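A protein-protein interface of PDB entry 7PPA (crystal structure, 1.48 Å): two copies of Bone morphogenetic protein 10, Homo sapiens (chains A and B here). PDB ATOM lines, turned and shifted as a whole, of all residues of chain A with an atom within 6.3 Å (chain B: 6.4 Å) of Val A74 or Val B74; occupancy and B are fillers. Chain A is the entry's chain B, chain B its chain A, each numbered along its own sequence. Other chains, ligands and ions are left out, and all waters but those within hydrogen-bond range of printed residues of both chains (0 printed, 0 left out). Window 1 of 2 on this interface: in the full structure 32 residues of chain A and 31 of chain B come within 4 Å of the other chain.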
ATOM      1  N   CYS A   7      19.458  -8.990 -16.611  1.00  0.00           N
ATOM      2  CA  CYS A   7      20.435  -9.184 -15.518  1.00  0.00           C
ATOM      3  C   CYS A   7      21.853  -9.066 -16.090  1.00  0.00           C
ATOM      4  O   CYS A   7      22.205  -9.858 -16.993  1.00  0.00           O
ATOM      5  CB  CYS A   7      20.205 -10.550 -14.893  1.00  0.00           C
ATOM      6  SG  CYS A   7      21.463 -10.974 -13.645  1.00  0.00           S
ATOM      7  N   CYS A  36      25.064  -6.189  -9.743  1.00  0.00           N
ATOM      8  CA  CYS A  36      24.232  -6.960 -10.670  1.00  0.00           C
ATOM      9  C   CYS A  36      22.855  -6.300 -10.695  1.00  0.00           C
ATOM     10  O   CYS A  36      22.283  -6.115  -9.610  1.00  0.00           O
ATOM     11  CB  CYS A  36      24.183  -8.414 -10.230  1.00  0.00           C
ATOM     12  SG  CYS A  36      25.838  -9.161 -10.312  1.00  0.00           S
ATOM     13  N   CYS A  40      15.534 -11.241 -14.469  1.00  0.00           N
ATOM     14  CA  CYS A  40      15.695 -12.646 -14.850  1.00  0.00           C
ATOM     15  C   CYS A  40      14.373 -13.158 -15.426  1.00  0.00           C
ATOM     16  O   CYS A  40      13.412 -13.378 -14.632  1.00  0.00           O
ATOM     17  CB  CYS A  40      16.027 -13.450 -13.598  1.00  0.00           C
ATOM     18  SG  CYS A  40      17.621 -13.003 -12.907  1.00  0.00           S
ATOM     19  N   ALA A  71      13.182 -15.171 -10.145  1.00  0.00           N
ATOM     20  CA  ALA A  71      14.592 -15.410  -9.853  1.00  0.00           C
ATOM     21  C   ALA A  71      15.275 -14.048  -9.762  1.00  0.00           C
ATOM     22  O   ALA A  71      14.809 -13.081 -10.369  1.00  0.00           O
ATOM     23  CB  ALA A  71      15.260 -16.275 -10.907  1.00  0.00           C
ATOM     24  N   CYS A  72      16.295 -13.931  -8.916  1.00  0.00           N
ATOM     25  CA  CYS A  72      16.958 -12.643  -8.618  1.00  0.00           C
ATOM     26  C   CYS A  72      18.307 -12.533  -9.330  1.00  0.00           C
ATOM     27  O   CYS A  72      19.049 -13.533  -9.336  1.00  0.00           O
ATOM     28  CB  CYS A  72      17.129 -12.465  -7.116  1.00  0.00           C
ATOM     29  SG  CYS A  72      17.283 -10.706  -6.743  1.00  0.00           S
ATOM     30  N   CYS A  73      18.588 -11.326  -9.827  1.00  0.00           N
ATOM     31  CA  CYS A  73      19.905 -11.048 -10.446  1.00  0.00           C
ATOM     32  C   CYS A  73      20.912 -10.712  -9.337  1.00  0.00           C
ATOM     33  O   CYS A  73      20.753  -9.699  -8.648  1.00  0.00           O
ATOM     34  CB  CYS A  73      19.694  -9.970 -11.479  1.00  0.00           C
ATOM     35  SG  CYS A  73      21.201  -9.425 -12.265  1.00  0.00           S
ATOM     36  N   VAL A  74      21.896 -11.595  -9.115  1.00  0.00           N
ATOM     37  CA  VAL A  74      22.888 -11.466  -8.007  1.00  0.00           C
ATOM     38  C   VAL A  74      24.291 -11.816  -8.484  1.00  0.00           C
ATOM     39  O   VAL A  74      24.492 -12.439  -9.517  1.00  0.00           O
ATOM     40  CB  VAL A  74      22.534 -12.377  -6.824  1.00  0.00           C
ATOM     41  CG1 VAL A  74      21.229 -11.919  -6.128  1.00  0.00           C
ATOM     42  CG2 VAL A  74      22.393 -13.804  -7.271  1.00  0.00           C
ATOM     43  N   PRO A  75      25.320 -11.361  -7.735  1.00  0.00           N
ATOM     44  CA  PRO A  75      26.671 -11.743  -8.048  1.00  0.00           C
ATOM     45  C   PRO A  75      26.769 -13.266  -7.871  1.00  0.00           C
ATOM     46  O   PRO A  75      26.305 -13.820  -6.872  1.00  0.00           O
ATOM     47  CB  PRO A  75      27.532 -10.961  -7.055  1.00  0.00           C
ATOM     48  CG  PRO A  75      26.639  -9.845  -6.556  1.00  0.00           C
ATOM     49  CD  PRO A  75      25.257 -10.451  -6.577  1.00  0.00           C
ATOM     50  N   THR A  76      27.403 -13.881  -8.848  1.00  0.00           N
ATOM     51  CA  THR A  76      27.678 -15.330  -8.854  1.00  0.00           C
ATOM     52  C   THR A  76      29.174 -15.620  -8.870  1.00  0.00           C
ATOM     53  O   THR A  76      29.502 -16.775  -8.553  1.00  0.00           O
ATOM     54  CB  THR A  76      26.978 -16.001 -10.014  1.00  0.00           C
ATOM     55  OG1 THR A  76      27.385 -15.366 -11.237  1.00  0.00           O
ATOM     56  CG2 THR A  76      25.470 -15.964  -9.791  1.00  0.00           C
ATOM     57  N   LYS A  77      30.024 -14.630  -9.064  1.00  0.00           N
ATOM     58  CA  LYS A  77      31.472 -14.809  -8.847  1.00  0.00           C
ATOM     59  C   LYS A  77      31.983 -13.460  -8.333  1.00  0.00           C
ATOM     60  O   LYS A  77      31.649 -12.425  -8.957  1.00  0.00           O
ATOM     61  CB  LYS A  77      32.198 -15.243 -10.108  1.00  0.00           C
ATOM     62  CG  LYS A  77      33.621 -15.707  -9.861  1.00  0.00           C
ATOM     63  CD  LYS A  77      34.400 -16.086 -11.117  1.00  0.00           C
ATOM     64  CE  LYS A  77      35.694 -16.793 -10.782  1.00  0.00           C
ATOM     65  NZ  LYS A  77      36.557 -15.998  -9.874  1.00  0.00           N
ATOM     66  N   VAL A 102      32.476  -7.732  -8.084  1.00  0.00           N
ATOM     67  CA  VAL A 102      31.671  -8.661  -8.923  1.00  0.00           C
ATOM     68  C   VAL A 102      32.477  -8.960 -10.186  1.00  0.00           C
ATOM     69  O   VAL A 102      32.838  -8.020 -10.865  1.00  0.00           O
ATOM     70  CB  VAL A 102      30.306  -8.065  -9.302  1.00  0.00           C
ATOM     71  CG1 VAL A 102      29.555  -9.054 -10.197  1.00  0.00           C
ATOM     72  CG2 VAL A 102      29.500  -7.729  -8.054  1.00  0.00           C
ATOM     73  N   GLU A 104      31.032 -11.851 -12.101  1.00  0.00           N
ATOM     74  CA  GLU A 104      29.946 -12.481 -12.882  1.00  0.00           C
ATOM     75  C   GLU A 104      28.628 -12.296 -12.147  1.00  0.00           C
ATOM     76  O   GLU A 104      28.635 -12.296 -10.893  1.00  0.00           O
ATOM     77  CB  GLU A 104      30.185 -13.976 -13.058  1.00  0.00           C
ATOM     78  CG  GLU A 104      31.475 -14.293 -13.775  1.00  0.00           C
ATOM     79  CD  GLU A 104      31.819 -15.742 -13.982  1.00  0.00           C
ATOM     80  OE1 GLU A 104      30.971 -16.615 -13.666  1.00  0.00           O
ATOM     81  OE2 GLU A 104      32.937 -15.975 -14.473  1.00  0.00           O
ATOM     82  N   CYS A 105      27.554 -12.168 -12.936  1.00  0.00           N
ATOM     83  CA  CYS A 105      26.173 -11.999 -12.422  1.00  0.00           C
ATOM     84  C   CYS A 105      25.387 -13.202 -12.932  1.00  0.00           C
ATOM     85  O   CYS A 105      25.760 -13.808 -13.962  1.00  0.00           O
ATOM     86  CB  CYS A 105      25.508 -10.721 -12.914  1.00  0.00           C
ATOM     87  SG  CYS A 105      26.303  -9.230 -12.308  1.00  0.00           S
ATOM     88  N   GLY A 106      24.369 -13.610 -12.201  1.00  0.00           N
ATOM     89  CA  GLY A 106      23.465 -14.666 -12.661  1.00  0.00           C
ATOM     90  C   GLY A 106      22.128 -14.576 -11.943  1.00  0.00           C
ATOM     91  O   GLY A 106      21.915 -13.736 -11.109  1.00  0.00           O
ATOM     92  N   CYS A 107      21.281 -15.513 -12.296  1.00  0.00           N
ATOM     93  CA  CYS A 107      19.895 -15.644 -11.819  1.00  0.00           C
ATOM     94  C   CYS A 107      19.826 -16.772 -10.766  1.00  0.00           C
ATOM     95  O   CYS A 107      20.206 -17.885 -11.095  1.00  0.00           O
ATOM     96  CB  CYS A 107      18.932 -15.824 -12.992  1.00  0.00           C
ATOM     97  SG  CYS A 107      18.868 -14.309 -13.989  1.00  0.00           S
ATOM     98  N   ARG A 108      19.334 -16.485  -9.557  1.00  0.00           N
ATOM     99  CA  ARG A 108      19.312 -17.450  -8.423  1.00  0.00           C
ATOM    100  C   ARG A 108      17.941 -17.461  -7.745  1.00  0.00           C
ATOM    101  O   ARG A 108      17.652 -18.530  -7.144  1.00  0.00           O
ATOM    102  CB  ARG A 108      20.466 -17.210  -7.457  1.00  0.00           C
ATOM    103  CG  ARG A 108      21.858 -17.375  -8.060  1.00  0.00           C
ATOM    104  CD  ARG A 108      22.118 -18.812  -8.457  1.00  0.00           C
ATOM    105  NE  ARG A 108      23.482 -19.043  -8.936  1.00  0.00           N
ATOM    106  CZ  ARG A 108      23.910 -18.885 -10.182  1.00  0.00           C
ATOM    107  NH1 ARG A 108      23.128 -18.373 -11.147  1.00  0.00           N
ATOM    108  NH2 ARG A 108      25.152 -19.222 -10.436  1.00  0.00           N
ATOM    109  OXT ARG A 108      17.230 -16.391  -7.830  1.00  0.00           O
ATOM    110  N   CYS B   7      14.550 -11.738   5.109  1.00  0.00           N
ATOM    111  CA  CYS B   7      14.902 -12.831   4.195  1.00  0.00           C
ATOM    112  C   CYS B   7      14.833 -14.179   4.927  1.00  0.00           C
ATOM    113  O   CYS B   7      15.520 -14.340   5.939  1.00  0.00           O
ATOM    114  CB  CYS B   7      16.325 -12.567   3.737  1.00  0.00           C
ATOM    115  SG  CYS B   7      16.916 -13.846   2.634  1.00  0.00           S
ATOM    116  N   CYS B  36      12.968 -18.435  -1.219  1.00  0.00           N
ATOM    117  CA  CYS B  36      13.525 -17.428  -0.295  1.00  0.00           C
ATOM    118  C   CYS B  36      12.754 -16.142  -0.504  1.00  0.00           C
ATOM    119  O   CYS B  36      12.729 -15.702  -1.658  1.00  0.00           O
ATOM    120  CB  CYS B  36      15.020 -17.226  -0.597  1.00  0.00           C
ATOM    121  SG  CYS B  36      15.958 -18.756  -0.268  1.00  0.00           S
ATOM    122  N   CYS B  40      16.514  -7.845   2.509  1.00  0.00           N
ATOM    123  CA  CYS B  40      17.871  -7.769   3.059  1.00  0.00           C
ATOM    124  C   CYS B  40      18.180  -6.293   3.345  1.00  0.00           C
ATOM    125  O   CYS B  40      18.278  -5.497   2.376  1.00  0.00           O
ATOM    126  CB  CYS B  40      18.837  -8.305   2.026  1.00  0.00           C
ATOM    127  SG  CYS B  40      18.627 -10.052   1.688  1.00  0.00           S
ATOM    128  N   ALA B  71      20.744  -5.602  -1.380  1.00  0.00           N
ATOM    129  CA  ALA B  71      21.140  -7.010  -1.526  1.00  0.00           C
ATOM    130  C   ALA B  71      19.851  -7.820  -1.696  1.00  0.00           C
ATOM    131  O   ALA B  71      18.790  -7.394  -1.293  1.00  0.00           O
ATOM    132  CB  ALA B  71      21.930  -7.417  -0.314  1.00  0.00           C
ATOM    133  N   CYS B  72      19.968  -8.962  -2.325  1.00  0.00           N
ATOM    134  CA  CYS B  72      18.819  -9.797  -2.707  1.00  0.00           C
ATOM    135  C   CYS B  72      18.739 -11.083  -1.880  1.00  0.00           C
ATOM    136  O   CYS B  72      19.785 -11.733  -1.623  1.00  0.00           O
ATOM    137  CB  CYS B  72      18.861 -10.159  -4.180  1.00  0.00           C
ATOM    138  SG  CYS B  72      17.192 -10.588  -4.730  1.00  0.00           S
ATOM    139  N   CYS B  73      17.526 -11.422  -1.471  1.00  0.00           N
ATOM    140  CA  CYS B  73      17.250 -12.676  -0.737  1.00  0.00           C
ATOM    141  C   CYS B  73      17.155 -13.828  -1.725  1.00  0.00           C
ATOM    142  O   CYS B  73      16.222 -13.816  -2.544  1.00  0.00           O
ATOM    143  CB  CYS B  73      16.015 -12.446   0.109  1.00  0.00           C
ATOM    144  SG  CYS B  73      15.579 -13.891   1.063  1.00  0.00           S
ATOM    145  N   VAL B  74      18.127 -14.743  -1.672  1.00  0.00           N
ATOM    146  CA  VAL B  74      18.262 -15.845  -2.658  1.00  0.00           C
ATOM    147  C   VAL B  74      18.637 -17.124  -1.955  1.00  0.00           C
ATOM    148  O   VAL B  74      19.148 -17.115  -0.824  1.00  0.00           O
ATOM    149  CB  VAL B  74      19.272 -15.528  -3.758  1.00  0.00           C
ATOM    150  CG1 VAL B  74      18.737 -14.471  -4.711  1.00  0.00           C
ATOM    151  CG2 VAL B  74      20.610 -15.156  -3.186  1.00  0.00           C
ATOM    152  N   PRO B  75      18.389 -18.283  -2.628  1.00  0.00           N
ATOM    153  CA  PRO B  75      18.895 -19.540  -2.092  1.00  0.00           C
ATOM    154  C   PRO B  75      20.403 -19.410  -2.079  1.00  0.00           C
ATOM    155  O   PRO B  75      20.983 -18.964  -3.090  1.00  0.00           O
ATOM    156  CB  PRO B  75      18.354 -20.590  -3.072  1.00  0.00           C
ATOM    157  CG  PRO B  75      17.177 -19.869  -3.721  1.00  0.00           C
ATOM    158  CD  PRO B  75      17.643 -18.473  -3.889  1.00  0.00           C
ATOM    159  N   THR B  76      20.979 -19.864  -0.989  1.00  0.00           N
ATOM    160  CA  THR B  76      22.450 -19.991  -0.825  1.00  0.00           C
ATOM    161  C   THR B  76      22.899 -21.433  -0.647  1.00  0.00           C
ATOM    162  O   THR B  76      24.063 -21.630  -0.696  1.00  0.00           O
ATOM    163  CB  THR B  76      22.883 -19.089   0.318  1.00  0.00           C
ATOM    164  OG1 THR B  76      22.139 -19.400   1.494  1.00  0.00           O
ATOM    165  CG2 THR B  76      22.691 -17.640  -0.079  1.00  0.00           C
ATOM    166  N   LYS B  77      22.000 -22.378  -0.408  1.00  0.00           N
ATOM    167  CA  LYS B  77      22.350 -23.801  -0.414  1.00  0.00           C
ATOM    168  C   LYS B  77      21.155 -24.529  -1.000  1.00  0.00           C
ATOM    169  O   LYS B  77      20.037 -24.291  -0.544  1.00  0.00           O
ATOM    170  CB  LYS B  77      22.693 -24.307   0.977  1.00  0.00           C
ATOM    171  CG  LYS B  77      23.430 -25.622   0.968  1.00  0.00           C
ATOM    172  CD  LYS B  77      23.785 -26.122   2.375  1.00  0.00           C
ATOM    173  CE  LYS B  77      24.678 -27.349   2.364  1.00  0.00           C
ATOM    174  NZ  LYS B  77      24.104 -28.414   1.520  1.00  0.00           N
ATOM    175  N   VAL B 102      15.630 -25.848  -1.771  1.00  0.00           N
ATOM    176  CA  VAL B 102      16.353 -24.866  -0.950  1.00  0.00           C
ATOM    177  C   VAL B 102      16.557 -25.458   0.446  1.00  0.00           C
ATOM    178  O   VAL B 102      15.569 -25.816   1.074  1.00  0.00           O
ATOM    179  CB  VAL B 102      15.613 -23.538  -0.862  1.00  0.00           C
ATOM    180  CG1 VAL B 102      16.397 -22.588   0.030  1.00  0.00           C
ATOM    181  CG2 VAL B 102      15.369 -22.931  -2.222  1.00  0.00           C
ATOM    182  N   GLU B 104      19.050 -23.425   2.462  1.00  0.00           N
ATOM    183  CA  GLU B 104      19.418 -22.151   3.139  1.00  0.00           C
ATOM    184  C   GLU B 104      19.151 -20.970   2.216  1.00  0.00           C
ATOM    185  O   GLU B 104      19.311 -21.110   0.991  1.00  0.00           O
ATOM    186  CB  GLU B 104      20.872 -22.134   3.606  1.00  0.00           C
ATOM    187  CG  GLU B 104      21.223 -23.304   4.495  1.00  0.00           C
ATOM    188  CD  GLU B 104      22.667 -23.491   4.909  1.00  0.00           C
ATOM    189  OE1 GLU B 104      23.492 -22.720   4.480  1.00  0.00           O
ATOM    190  OE2 GLU B 104      22.970 -24.446   5.642  1.00  0.00           O
ATOM    191  N   CYS B 105      18.758 -19.858   2.843  1.00  0.00           N
ATOM    192  CA  CYS B 105      18.528 -18.557   2.154  1.00  0.00           C
ATOM    193  C   CYS B 105      19.570 -17.593   2.707  1.00  0.00           C
ATOM    194  O   CYS B 105      20.086 -17.804   3.870  1.00  0.00           O
ATOM    195  CB  CYS B 105      17.138 -17.967   2.417  1.00  0.00           C
ATOM    196  SG  CYS B 105      15.853 -19.040   1.760  1.00  0.00           S
ATOM    197  N   GLY B 106      19.956 -16.638   1.887  1.00  0.00           N
ATOM    198  CA  GLY B 106      20.847 -15.558   2.349  1.00  0.00           C
ATOM    199  C   GLY B 106      20.725 -14.329   1.498  1.00  0.00           C
ATOM    200  O   GLY B 106      20.001 -14.298   0.528  1.00  0.00           O
ATOM    201  N   CYS B 107      21.580 -13.375   1.824  1.00  0.00           N
ATOM    202  CA  CYS B 107      21.610 -12.052   1.158  1.00  0.00           C
ATOM    203  C   CYS B 107      22.864 -11.948   0.266  1.00  0.00           C
ATOM    204  O   CYS B 107      23.984 -12.222   0.755  1.00  0.00           O
ATOM    205  CB  CYS B 107      21.553 -10.936   2.175  1.00  0.00           C
ATOM    206  SG  CYS B 107      19.975 -10.888   3.078  1.00  0.00           S
ATOM    207  N   ARG B 108      22.683 -11.664  -1.019  1.00  0.00           N
ATOM    208  CA  ARG B 108      23.788 -11.619  -2.010  1.00  0.00           C
ATOM    209  C   ARG B 108      23.684 -10.362  -2.876  1.00  0.00           C
ATOM    210  O   ARG B 108      24.789  -9.942  -3.341  1.00  0.00           O
ATOM    211  CB  ARG B 108      23.741 -12.899  -2.849  1.00  0.00           C
ATOM    212  CG  ARG B 108      23.974 -14.191  -2.061  1.00  0.00           C
ATOM    213  CD  ARG B 108      25.374 -14.296  -1.547  1.00  0.00           C
ATOM    214  NE  ARG B 108      25.702 -15.529  -0.829  1.00  0.00           N
ATOM    215  CZ  ARG B 108      25.408 -15.809   0.429  1.00  0.00           C
ATOM    216  NH1 ARG B 108      24.713 -14.965   1.176  1.00  0.00           N
ATOM    217  NH2 ARG B 108      25.775 -16.996   0.927  1.00  0.00           N
ATOM    218  OXT ARG B 108      22.610  -9.741  -3.014  1.00  0.00           O
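The side-chain sulfur (SG) of Cys A72 forms a disulfide with the side-chain sulfur (SG) of Cys B72, 2.0 Å away.
The backbone NH of Cys A72 lies within hydrogen-bond range of the chain-end carboxylate of Arg A108.
N of Val A74 lies within hydrogen-bond range of O of Gly A106.
SG of Cys B73 forms a disulfide with SG of Cys B7 (2.1 Å).
The side-chain sulfur (SG) of Cys B105 is disulfide-bonded to the side-chain sulfur (SG) of Cys B36, at 2.1 Å.
The side-chain sulfur (SG) of Cys A7 forms a disulfide with the side-chain sulfur (SG) of Cys A73, at 2.1 Å.
SG of Cys A36 forms a disulfide with SG of Cys A105 (2.1 Å).
Among the printed residues, merely in contact across the chains: Cys A72 with Val B74, Val A74 with Cys B72, Val A74 with Val B74, Pro A75 with Arg B108, Arg A108 with Val B74 and Arg A108 with Pro B75.
Printed residues of chain B within 4 Å of Cys A72: Cys B72 (2.0 Å) and Val B74 (3.5 Å).
Of the printed residues of chain A, Cys B72 touches Cys A72 (2.0 Å) and Val A74 (3.5 Å).
Of the printed residues of chain A, Arg B108 touches Pro A75 (3.3 Å).
Of the printed residues of chain B, Pro A75 touches Arg B108.
The nearest printed residue of chain B that does not touch Cys A72 is Cys B73 (4.9 Å).
Printed residues of chain A that touch a printed residue of chain B: Cys A72, Val A74, Pro A75 and Arg A108.
Hydrophobic or aromatic side chains of chain A within 4 Å of the printed part of chain B: Val A74 and Pro A75.
Among the printed residues, 7 pairs touch across the chains.
Among the printed residues, no Asp or Glu carboxylate lies within 4 Å of a Lys or Arg side-chain nitrogen of the other chain.
Cys A72 touches its own counterpart, Cys B72.
Cys A72 touches Val B74, and with the chains exchanged Val A74 touches Cys B72.
Val B74 touches its own counterpart, Val A74.
Arg A108 touches Val B74, but with the chains exchanged Val A74 does not touch Arg B108 (4.04 Å).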
